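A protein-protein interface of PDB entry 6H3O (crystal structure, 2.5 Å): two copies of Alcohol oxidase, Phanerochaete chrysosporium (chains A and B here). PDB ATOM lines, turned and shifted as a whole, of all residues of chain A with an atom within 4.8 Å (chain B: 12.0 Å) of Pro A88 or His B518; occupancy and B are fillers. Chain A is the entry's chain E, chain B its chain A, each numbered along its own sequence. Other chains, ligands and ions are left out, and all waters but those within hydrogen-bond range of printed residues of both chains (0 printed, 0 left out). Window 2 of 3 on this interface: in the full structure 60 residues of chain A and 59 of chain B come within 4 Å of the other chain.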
ATOM      1  N   MET A  59      21.006  -6.989   6.532  1.00  0.00           N
ATOM      2  CA  MET A  59      20.341  -5.770   7.003  1.00  0.00           C
ATOM      3  C   MET A  59      21.356  -4.731   7.524  1.00  0.00           C
ATOM      4  O   MET A  59      20.985  -3.782   8.241  1.00  0.00           O
ATOM      5  CB  MET A  59      19.301  -6.134   8.067  1.00  0.00           C
ATOM      6  CG  MET A  59      18.042  -6.692   7.442  1.00  0.00           C
ATOM      7  SD  MET A  59      17.220  -5.432   6.412  1.00  0.00           S
ATOM      8  CE  MET A  59      16.933  -6.370   4.912  1.00  0.00           C
ATOM      9  N   ARG A  61      23.334  -1.526   7.029  1.00  0.00           N
ATOM     10  CA  ARG A  61      23.482  -0.236   6.352  1.00  0.00           C
ATOM     11  C   ARG A  61      24.934   0.212   6.530  1.00  0.00           C
ATOM     12  O   ARG A  61      25.214   1.114   7.298  1.00  0.00           O
ATOM     13  CB  ARG A  61      22.491   0.791   6.907  1.00  0.00           C
ATOM     14  CG  ARG A  61      21.482   1.311   5.892  1.00  0.00           C
ATOM     15  CD  ARG A  61      20.146   1.697   6.517  1.00  0.00           C
ATOM     16  NE  ARG A  61      20.162   2.871   7.395  1.00  0.00           N
ATOM     17  CZ  ARG A  61      20.341   2.844   8.722  1.00  0.00           C
ATOM     18  NH1 ARG A  61      20.845   1.772   9.314  1.00  0.00           N
ATOM     19  NH2 ARG A  61      20.011   3.896   9.453  1.00  0.00           N
ATOM     20  N   ALA A  68      19.548  -5.304  -0.348  1.00  0.00           N
ATOM     21  CA  ALA A  68      18.327  -4.701   0.227  1.00  0.00           C
ATOM     22  C   ALA A  68      18.175  -3.242  -0.231  1.00  0.00           C
ATOM     23  O   ALA A  68      19.160  -2.538  -0.433  1.00  0.00           O
ATOM     24  CB  ALA A  68      18.392  -4.776   1.731  1.00  0.00           C
ATOM     25  N   THR A  69      16.926  -2.782  -0.379  1.00  0.00           N
ATOM     26  CA  THR A  69      16.651  -1.356  -0.594  1.00  0.00           C
ATOM     27  C   THR A  69      16.009  -0.813   0.687  1.00  0.00           C
ATOM     28  O   THR A  69      15.222  -1.533   1.323  1.00  0.00           O
ATOM     29  CB  THR A  69      15.807  -1.087  -1.852  1.00  0.00           C
ATOM     30  OG1 THR A  69      14.459  -0.808  -1.480  1.00  0.00           O
ATOM     31  CG2 THR A  69      15.820  -2.218  -2.852  1.00  0.00           C
ATOM     32  N   PHE A  70      16.363   0.432   1.055  1.00  0.00           N
ATOM     33  CA  PHE A  70      15.948   1.040   2.332  1.00  0.00           C
ATOM     34  C   PHE A  70      14.982   2.201   2.080  1.00  0.00           C
ATOM     35  O   PHE A  70      15.328   3.166   1.408  1.00  0.00           O
ATOM     36  CB  PHE A  70      17.168   1.492   3.132  1.00  0.00           C
ATOM     37  CG  PHE A  70      18.001   0.340   3.627  1.00  0.00           C
ATOM     38  CD1 PHE A  70      19.001  -0.197   2.839  1.00  0.00           C
ATOM     39  CD2 PHE A  70      17.756  -0.231   4.862  1.00  0.00           C
ATOM     40  CE1 PHE A  70      19.758  -1.265   3.284  1.00  0.00           C
ATOM     41  CE2 PHE A  70      18.518  -1.300   5.307  1.00  0.00           C
ATOM     42  CZ  PHE A  70      19.520  -1.815   4.516  1.00  0.00           C
ATOM     43  N   ILE A  86      12.137   2.982   9.403  1.00  0.00           N
ATOM     44  CA  ILE A  86      12.914   2.423   8.266  1.00  0.00           C
ATOM     45  C   ILE A  86      12.436   1.000   7.979  1.00  0.00           C
ATOM     46  O   ILE A  86      12.511   0.140   8.851  1.00  0.00           O
ATOM     47  CB  ILE A  86      14.432   2.393   8.532  1.00  0.00           C
ATOM     48  CG1 ILE A  86      15.035   3.797   8.643  1.00  0.00           C
ATOM     49  CG2 ILE A  86      15.120   1.557   7.456  1.00  0.00           C
ATOM     50  CD1 ILE A  86      16.524   3.822   8.950  1.00  0.00           C
ATOM     51  N   VAL A  87      12.031   0.762   6.728  1.00  0.00           N
ATOM     52  CA  VAL A  87      11.520  -0.512   6.286  1.00  0.00           C
ATOM     53  C   VAL A  87      12.379  -0.998   5.123  1.00  0.00           C
ATOM     54  O   VAL A  87      12.296  -0.464   4.025  1.00  0.00           O
ATOM     55  CB  VAL A  87      10.039  -0.400   5.893  1.00  0.00           C
ATOM     56  CG1 VAL A  87       9.519  -1.702   5.303  1.00  0.00           C
ATOM     57  CG2 VAL A  87       9.182   0.022   7.071  1.00  0.00           C
ATOM     58  N   PRO A  88      13.268  -1.993   5.335  1.00  0.00           N
ATOM     59  CA  PRO A  88      14.024  -2.601   4.244  1.00  0.00           C
ATOM     60  C   PRO A  88      13.224  -3.694   3.523  1.00  0.00           C
ATOM     61  O   PRO A  88      12.237  -4.195   4.043  1.00  0.00           O
ATOM     62  CB  PRO A  88      15.241  -3.239   4.945  1.00  0.00           C
ATOM     63  CG  PRO A  88      15.176  -2.733   6.375  1.00  0.00           C
ATOM     64  CD  PRO A  88      13.697  -2.521   6.638  1.00  0.00           C
ATOM     65  N   CYS A  89      13.690  -4.063   2.332  1.00  0.00           N
ATOM     66  CA  CYS A  89      13.232  -5.243   1.657  1.00  0.00           C
ATOM     67  C   CYS A  89      14.310  -5.677   0.670  1.00  0.00           C
ATOM     68  O   CYS A  89      15.181  -4.891   0.300  1.00  0.00           O
ATOM     69  CB  CYS A  89      11.924  -4.997   0.915  1.00  0.00           C
ATOM     70  SG  CYS A  89      12.085  -3.784  -0.422  1.00  0.00           S
ATOM     71  N   ALA A  90      14.208  -6.932   0.237  1.00  0.00           N
ATOM     72  CA  ALA A  90      15.203  -7.549  -0.611  1.00  0.00           C
ATOM     73  C   ALA A  90      15.375  -6.744  -1.903  1.00  0.00           C
ATOM     74  O   ALA A  90      14.451  -6.059  -2.364  1.00  0.00           O
ATOM     75  CB  ALA A  90      14.817  -8.979  -0.896  1.00  0.00           C
ATOM     76  N   GLU A 557       9.549  -1.970  15.199  1.00  0.00           N
ATOM     77  CA  GLU A 557      10.187  -2.050  13.911  1.00  0.00           C
ATOM     78  C   GLU A 557       9.298  -2.867  12.967  1.00  0.00           C
ATOM     79  O   GLU A 557       8.387  -3.564  13.420  1.00  0.00           O
ATOM     80  CB  GLU A 557      11.566  -2.691  14.091  1.00  0.00           C
ATOM     81  CG  GLU A 557      12.676  -1.942  13.382  1.00  0.00           C
ATOM     82  CD  GLU A 557      13.012  -0.583  13.967  1.00  0.00           C
ATOM     83  OE1 GLU A 557      13.606  -0.549  15.061  1.00  0.00           O
ATOM     84  OE2 GLU A 557      12.687   0.433  13.323  1.00  0.00           O
ATOM     85  N   THR A 558       9.576  -2.768  11.662  1.00  0.00           N
ATOM     86  CA  THR A 558       9.032  -3.698  10.668  1.00  0.00           C
ATOM     87  C   THR A 558       9.455  -5.128  11.040  1.00  0.00           C
ATOM     88  O   THR A 558      10.360  -5.322  11.860  1.00  0.00           O
ATOM     89  CB  THR A 558       9.489  -3.341   9.245  1.00  0.00           C
ATOM     90  OG1 THR A 558       8.913  -4.302   8.358  1.00  0.00           O
ATOM     91  CG2 THR A 558      10.992  -3.332   9.054  1.00  0.00           C
ATOM     92  N   TRP A 560       9.467  -7.138   8.097  1.00  0.00           N
ATOM     93  CA  TRP A 560       9.688  -7.447   6.676  1.00  0.00           C
ATOM     94  C   TRP A 560       8.512  -8.233   6.089  1.00  0.00           C
ATOM     95  O   TRP A 560       8.595  -8.706   4.950  1.00  0.00           O
ATOM     96  CB  TRP A 560      11.007  -8.209   6.483  1.00  0.00           C
ATOM     97  CG  TRP A 560      12.200  -7.501   7.045  1.00  0.00           C
ATOM     98  CD1 TRP A 560      12.772  -6.359   6.565  1.00  0.00           C
ATOM     99  CD2 TRP A 560      12.972  -7.883   8.199  1.00  0.00           C
ATOM    100  NE1 TRP A 560      13.851  -6.010   7.331  1.00  0.00           N
ATOM    101  CE2 TRP A 560      14.000  -6.926   8.341  1.00  0.00           C
ATOM    102  CE3 TRP A 560      12.905  -8.937   9.120  1.00  0.00           C
ATOM    103  CZ2 TRP A 560      14.946  -7.002   9.362  1.00  0.00           C
ATOM    104  CZ3 TRP A 560      13.842  -9.010  10.128  1.00  0.00           C
ATOM    105  CH2 TRP A 560      14.849  -8.054  10.245  1.00  0.00           C
ATOM    106  N   THR B 483      24.803   6.842  24.506  1.00  0.00           N
ATOM    107  CA  THR B 483      23.377   7.008  24.802  1.00  0.00           C
ATOM    108  C   THR B 483      23.034   6.332  26.136  1.00  0.00           C
ATOM    109  O   THR B 483      22.385   6.937  26.987  1.00  0.00           O
ATOM    110  CB  THR B 483      22.508   6.433  23.677  1.00  0.00           C
ATOM    111  OG1 THR B 483      23.050   5.148  23.388  1.00  0.00           O
ATOM    112  CG2 THR B 483      22.496   7.268  22.417  1.00  0.00           C
ATOM    113  N   ASP B 499      24.958   8.925  19.108  1.00  0.00           N
ATOM    114  CA  ASP B 499      25.897   7.863  19.486  1.00  0.00           C
ATOM    115  C   ASP B 499      26.905   7.661  18.344  1.00  0.00           C
ATOM    116  O   ASP B 499      27.012   8.515  17.463  1.00  0.00           O
ATOM    117  CB  ASP B 499      25.137   6.589  19.866  1.00  0.00           C
ATOM    118  CG  ASP B 499      25.776   5.761  20.976  1.00  0.00           C
ATOM    119  OD1 ASP B 499      26.903   5.262  20.764  1.00  0.00           O
ATOM    120  OD2 ASP B 499      25.123   5.592  22.032  1.00  0.00           O
ATOM    121  N   ILE B 500      27.640   6.541  18.377  1.00  0.00           N
ATOM    122  CA  ILE B 500      28.712   6.259  17.425  1.00  0.00           C
ATOM    123  C   ILE B 500      28.193   6.341  15.979  1.00  0.00           C
ATOM    124  O   ILE B 500      27.113   5.854  15.654  1.00  0.00           O
ATOM    125  CB  ILE B 500      29.385   4.903  17.728  1.00  0.00           C
ATOM    126  CG1 ILE B 500      30.634   4.691  16.868  1.00  0.00           C
ATOM    127  CG2 ILE B 500      28.405   3.750  17.586  1.00  0.00           C
ATOM    128  CD1 ILE B 500      31.589   3.656  17.412  1.00  0.00           C
ATOM    129  N   ASP B 501      28.992   6.993  15.122  1.00  0.00           N
ATOM    130  CA  ASP B 501      28.783   7.062  13.668  1.00  0.00           C
ATOM    131  C   ASP B 501      29.127   5.712  13.021  1.00  0.00           C
ATOM    132  O   ASP B 501      29.844   4.886  13.601  1.00  0.00           O
ATOM    133  CB  ASP B 501      29.622   8.178  13.038  1.00  0.00           C
ATOM    134  CG  ASP B 501      31.124   8.012  13.228  1.00  0.00           C
ATOM    135  OD1 ASP B 501      31.580   8.086  14.396  1.00  0.00           O
ATOM    136  OD2 ASP B 501      31.831   7.825  12.207  1.00  0.00           O
ATOM    137  N   ILE B 502      28.633   5.508  11.797  1.00  0.00           N
ATOM    138  CA  ILE B 502      28.697   4.194  11.145  1.00  0.00           C
ATOM    139  C   ILE B 502      30.151   3.835  10.792  1.00  0.00           C
ATOM    140  O   ILE B 502      30.519   2.666  10.885  1.00  0.00           O
ATOM    141  CB  ILE B 502      27.747   4.090   9.929  1.00  0.00           C
ATOM    142  CG1 ILE B 502      27.809   2.710   9.268  1.00  0.00           C
ATOM    143  CG2 ILE B 502      27.990   5.196   8.919  1.00  0.00           C
ATOM    144  CD1 ILE B 502      27.274   1.582  10.129  1.00  0.00           C
ATOM    145  N   ALA B 505      31.990   2.597  13.846  1.00  0.00           N
ATOM    146  CA  ALA B 505      31.496   1.261  14.136  1.00  0.00           C
ATOM    147  C   ALA B 505      32.198   0.243  13.230  1.00  0.00           C
ATOM    148  O   ALA B 505      32.745  -0.737  13.716  1.00  0.00           O
ATOM    149  CB  ALA B 505      30.000   1.212  13.957  1.00  0.00           C
ATOM    150  N   LYS B 506      32.185   0.506  11.917  1.00  0.00           N
ATOM    151  CA  LYS B 506      32.759  -0.394  10.901  1.00  0.00           C
ATOM    152  C   LYS B 506      34.241  -0.652  11.192  1.00  0.00           C
ATOM    153  O   LYS B 506      34.744  -1.738  10.904  1.00  0.00           O
ATOM    154  CB  LYS B 506      32.573   0.172   9.489  1.00  0.00           C
ATOM    155  CG  LYS B 506      31.165   0.019   8.922  1.00  0.00           C
ATOM    156  CD  LYS B 506      30.863   0.936   7.762  1.00  0.00           C
ATOM    157  CE  LYS B 506      31.536   0.497   6.480  1.00  0.00           C
ATOM    158  NZ  LYS B 506      31.806   1.649   5.589  1.00  0.00           N
ATOM    159  N   GLY B 512      32.230  -8.106  11.373  1.00  0.00           N
ATOM    160  CA  GLY B 512      30.961  -8.357  12.082  1.00  0.00           C
ATOM    161  C   GLY B 512      29.742  -8.096  11.206  1.00  0.00           C
ATOM    162  O   GLY B 512      29.733  -7.163  10.406  1.00  0.00           O
ATOM    163  N   LEU B 513      28.699  -8.923  11.381  1.00  0.00           N
ATOM    164  CA  LEU B 513      27.487  -8.914  10.530  1.00  0.00           C
ATOM    165  C   LEU B 513      26.387  -8.001  11.106  1.00  0.00           C
ATOM    166  O   LEU B 513      25.399  -7.709  10.424  1.00  0.00           O
ATOM    167  CB  LEU B 513      26.918 -10.334  10.397  1.00  0.00           C
ATOM    168  CG  LEU B 513      27.889 -11.499  10.168  1.00  0.00           C
ATOM    169  CD1 LEU B 513      27.151 -12.665   9.513  1.00  0.00           C
ATOM    170  CD2 LEU B 513      29.098 -11.111   9.325  1.00  0.00           C
ATOM    171  N   THR B 514      26.604  -7.576  12.354  1.00  0.00           N
ATOM    172  CA  THR B 514      25.662  -6.875  13.209  1.00  0.00           C
ATOM    173  C   THR B 514      25.726  -5.356  12.982  1.00  0.00           C
ATOM    174  O   THR B 514      24.744  -4.647  13.195  1.00  0.00           O
ATOM    175  CB  THR B 514      26.023  -7.212  14.658  1.00  0.00           C
ATOM    176  OG1 THR B 514      25.376  -6.287  15.524  1.00  0.00           O
ATOM    177  CG2 THR B 514      27.519  -7.160  14.881  1.00  0.00           C
ATOM    178  N   VAL B 515      26.901  -4.874  12.560  1.00  0.00           N
ATOM    179  CA  VAL B 515      27.224  -3.441  12.485  1.00  0.00           C
ATOM    180  C   VAL B 515      26.420  -2.802  11.346  1.00  0.00           C
ATOM    181  O   VAL B 515      26.654  -3.107  10.178  1.00  0.00           O
ATOM    182  CB  VAL B 515      28.732  -3.187  12.288  1.00  0.00           C
ATOM    183  CG1 VAL B 515      29.023  -1.716  12.034  1.00  0.00           C
ATOM    184  CG2 VAL B 515      29.563  -3.688  13.459  1.00  0.00           C
ATOM    185  N   GLY B 516      25.505  -1.894  11.711  1.00  0.00           N
ATOM    186  CA  GLY B 516      24.759  -1.052  10.767  1.00  0.00           C
ATOM    187  C   GLY B 516      23.312  -1.483  10.634  1.00  0.00           C
ATOM    188  O   GLY B 516      22.554  -0.910   9.849  1.00  0.00           O
ATOM    189  N   ILE B 517      22.942  -2.516  11.398  1.00  0.00           N
ATOM    190  CA  ILE B 517      21.579  -2.981  11.485  1.00  0.00           C
ATOM    191  C   ILE B 517      20.801  -1.983  12.348  1.00  0.00           C
ATOM    192  O   ILE B 517      21.056  -1.874  13.545  1.00  0.00           O
ATOM    193  CB  ILE B 517      21.516  -4.413  12.050  1.00  0.00           C
ATOM    194  CG1 ILE B 517      22.253  -5.399  11.140  1.00  0.00           C
ATOM    195  CG2 ILE B 517      20.073  -4.833  12.305  1.00  0.00           C
ATOM    196  CD1 ILE B 517      21.994  -6.855  11.454  1.00  0.00           C
ATOM    197  N   HIS B 518      19.869  -1.273  11.703  1.00  0.00           N
ATOM    198  CA  HIS B 518      19.008  -0.303  12.335  1.00  0.00           C
ATOM    199  C   HIS B 518      18.074  -1.006  13.330  1.00  0.00           C
ATOM    200  O   HIS B 518      17.727  -0.435  14.383  1.00  0.00           O
ATOM    201  CB  HIS B 518      18.237   0.506  11.275  1.00  0.00           C
ATOM    202  CG  HIS B 518      16.941  -0.102  10.845  1.00  0.00           C
ATOM    203  ND1 HIS B 518      16.835  -0.904   9.731  1.00  0.00           N
ATOM    204  CD2 HIS B 518      15.702  -0.036  11.383  1.00  0.00           C
ATOM    205  CE1 HIS B 518      15.586  -1.304   9.600  1.00  0.00           C
ATOM    206  NE2 HIS B 518      14.870  -0.785  10.602  1.00  0.00           N
ATOM    207  N   MET B 519      17.671  -2.238  12.996  1.00  0.00           N
ATOM    208  CA  MET B 519      16.561  -2.925  13.675  1.00  0.00           C
ATOM    209  C   MET B 519      16.718  -2.805  15.194  1.00  0.00           C
ATOM    210  O   MET B 519      17.643  -3.360  15.777  1.00  0.00           O
ATOM    211  CB  MET B 519      16.493  -4.400  13.276  1.00  0.00           C
ATOM    212  CG  MET B 519      15.956  -4.614  11.868  1.00  0.00           C
ATOM    213  SD  MET B 519      14.149  -4.453  11.704  1.00  0.00           S
ATOM    214  CE  MET B 519      13.581  -5.797  12.750  1.00  0.00           C
ATOM    215  N   GLY B 520      15.806  -2.044  15.805  1.00  0.00           N
ATOM    216  CA  GLY B 520      15.806  -1.787  17.241  1.00  0.00           C
ATOM    217  C   GLY B 520      15.786  -0.303  17.560  1.00  0.00           C
ATOM    218  O   GLY B 520      15.178   0.098  18.548  1.00  0.00           O
ATOM    219  N   SER B 521      16.455   0.497  16.722  1.00  0.00           N
ATOM    220  CA  SER B 521      16.517   1.953  16.877  1.00  0.00           C
ATOM    221  C   SER B 521      17.065   2.309  18.271  1.00  0.00           C
ATOM    222  O   SER B 521      16.525   3.175  18.962  1.00  0.00           O
ATOM    223  CB  SER B 521      15.163   2.578  16.631  1.00  0.00           C
ATOM    224  OG  SER B 521      14.616   2.157  15.390  1.00  0.00           O
ATOM    225  N   TRP B 522      18.153   1.630  18.661  1.00  0.00           N
ATOM    226  CA  TRP B 522      18.754   1.718  20.001  1.00  0.00           C
ATOM    227  C   TRP B 522      19.592   2.992  20.181  1.00  0.00           C
ATOM    228  O   TRP B 522      19.812   3.418  21.323  1.00  0.00           O
ATOM    229  CB  TRP B 522      19.612   0.477  20.273  1.00  0.00           C
ATOM    230  CG  TRP B 522      18.830  -0.799  20.252  1.00  0.00           C
ATOM    231  CD1 TRP B 522      19.059  -1.902  19.480  1.00  0.00           C
ATOM    232  CD2 TRP B 522      17.668  -1.092  21.048  1.00  0.00           C
ATOM    233  NE1 TRP B 522      18.122  -2.863  19.751  1.00  0.00           N
ATOM    234  CE2 TRP B 522      17.256  -2.393  20.705  1.00  0.00           C
ATOM    235  CE3 TRP B 522      16.944  -0.387  22.013  1.00  0.00           C
ATOM    236  CZ2 TRP B 522      16.154  -2.997  21.303  1.00  0.00           C
ATOM    237  CZ3 TRP B 522      15.854  -0.985  22.602  1.00  0.00           C
ATOM    238  CH2 TRP B 522      15.466  -2.275  22.250  1.00  0.00           C
ATOM    239  N   HIS B 523      20.086   3.557  19.069  1.00  0.00           N
ATOM    240  CA  HIS B 523      20.880   4.778  19.077  1.00  0.00           C
ATOM    241  C   HIS B 523      20.572   5.619  17.830  1.00  0.00           C
ATOM    242  O   HIS B 523      20.345   5.074  16.762  1.00  0.00           O
ATOM    243  CB  HIS B 523      22.369   4.420  19.186  1.00  0.00           C
ATOM    244  CG  HIS B 523      22.964   3.871  17.929  1.00  0.00           C
ATOM    245  ND1 HIS B 523      22.726   2.578  17.498  1.00  0.00           N
ATOM    246  CD2 HIS B 523      23.780   4.434  17.010  1.00  0.00           C
ATOM    247  CE1 HIS B 523      23.372   2.371  16.367  1.00  0.00           C
ATOM    248  NE2 HIS B 523      24.025   3.494  16.046  1.00  0.00           N
ATOM    249  N   GLN B 524      20.556   6.947  17.996  1.00  0.00           N
ATOM    250  CA  GLN B 524      20.624   7.903  16.887  1.00  0.00           C
ATOM    251  C   GLN B 524      22.093   8.108  16.524  1.00  0.00           C
ATOM    252  O   GLN B 524      22.823   8.771  17.252  1.00  0.00           O
ATOM    253  CB  GLN B 524      20.003   9.249  17.274  1.00  0.00           C
ATOM    254  CG  GLN B 524      18.483   9.286  17.190  1.00  0.00           C
ATOM    255  CD  GLN B 524      17.854  10.181  18.236  1.00  0.00           C
ATOM    256  OE1 GLN B 524      16.809   9.864  18.808  1.00  0.00           O
ATOM    257  NE2 GLN B 524      18.487  11.313  18.513  1.00  0.00           N
ATOM    258  N   PRO B 525      22.597   7.556  15.403  1.00  0.00           N
ATOM    259  CA  PRO B 525      24.023   7.658  15.095  1.00  0.00           C
ATOM    260  C   PRO B 525      24.501   9.086  14.785  1.00  0.00           C
ATOM    261  O   PRO B 525      23.762   9.878  14.198  1.00  0.00           O
ATOM    262  CB  PRO B 525      24.194   6.752  13.865  1.00  0.00           C
ATOM    263  CG  PRO B 525      22.823   6.706  13.234  1.00  0.00           C
ATOM    264  CD  PRO B 525      21.850   6.799  14.391  1.00  0.00           C
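The backbone carbonyl oxygen (O) of Gly B516 is in hydrogen-bond range of the backbone NH (N) of Arg A61 (3.0 Å). A ring nitrogen (NE2) of His B518 is in hydrogen-bond range of the backbone carbonyl oxygen (O) of Ile A86 (3.1 Å). The backbone NH (N) of Gly B520 is in hydrogen-bond range of the side-chain carboxylate (OE1) of Glu A557 (2.8 Å). The side-chain carboxylate (OE1) of Glu A557 lies within hydrogen-bond range of the side-chain hydroxyl (OG) of Ser B521, at 2.9 Å.
SD of Met A59 is in hydrogen-bond range of NE1 of Trp A560 (3.5 Å). OG1 of Thr A558 lies within hydrogen-bond range of N of Trp A560 (2.9 Å).
Among the printed residues, merely in contact across the chains: Glu A557 with Met B519 (3.4 Å), Thr A558 with Met B519 (3.4 Å), Met A59 with Ile B517 (3.4 Å), Arg A61 with His B518 (3.5 Å), Arg A61 with Ile B502 (3.5 Å), Pro A88 with His B518 (3.6 Å), Trp A560 with Met B519 (3.6 Å), Glu A557 with His B518 (3.6 Å) and Met A59 with Gly B516 (3.6 Å).
No residue of chain B comes within 4 Å of Ala A68. No residue of chain B comes within 4 Å of Phe A70. Of the printed residues of chain B, Ile A86 touches His B518. Of the printed residues of chain B, Pro A88 touches His B518. Ala A90 touches none of the printed residues of chain B. Of chain B, only His B518 (3.6 Å), Met B519 (3.4 Å), Gly B520 (2.8 Å) and Ser B521 (2.9 Å) come within 4 Å of Glu A557. Thr A558 touches just one residue of chain B: Met B519 (3.4 Å). Trp A560 touches just one residue of chain B: Met B519 (3.6 Å). Of the printed residues of chain A, Ile B502 touches Arg A61 (3.5 Å). Of the printed residues of chain A, Gly B516 touches Met A59 (3.6 Å) and Arg A61 (3.0 Å). Printed residues of chain A within 4 Å of Ile B517: Met A59. His B518 touches four residues of chain A. Of the printed residues of chain A, Met B519 touches Glu A557, Thr A558 and Trp A560. Of the printed residues of chain A, Ser B521 touches Glu A557 (2.9 Å). The nearest printed residue of chain A that does not touch Ile B502 is Met A59 (8.5 Å).
Of the 13 printed residues of chain A, 7 touch a printed residue of chain B. Along chain A the printed residues that touch a printed residue of chain B span positions 59 to 560. Hydrophobic or aromatic side chains of chain B that line the printed part of chain A: Ile B502, Ile B517, His B518 and Met B519. Along chain B the printed residues that touch a printed residue of chain A span positions 502 to 521. Among the printed residues, 13 pairs touch across the chains. Among the printed residues, no Asp or Glu carboxylate lies within 4 Å of a Lys or Arg side-chain nitrogen of the other chain.
No position is printed for both chains.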
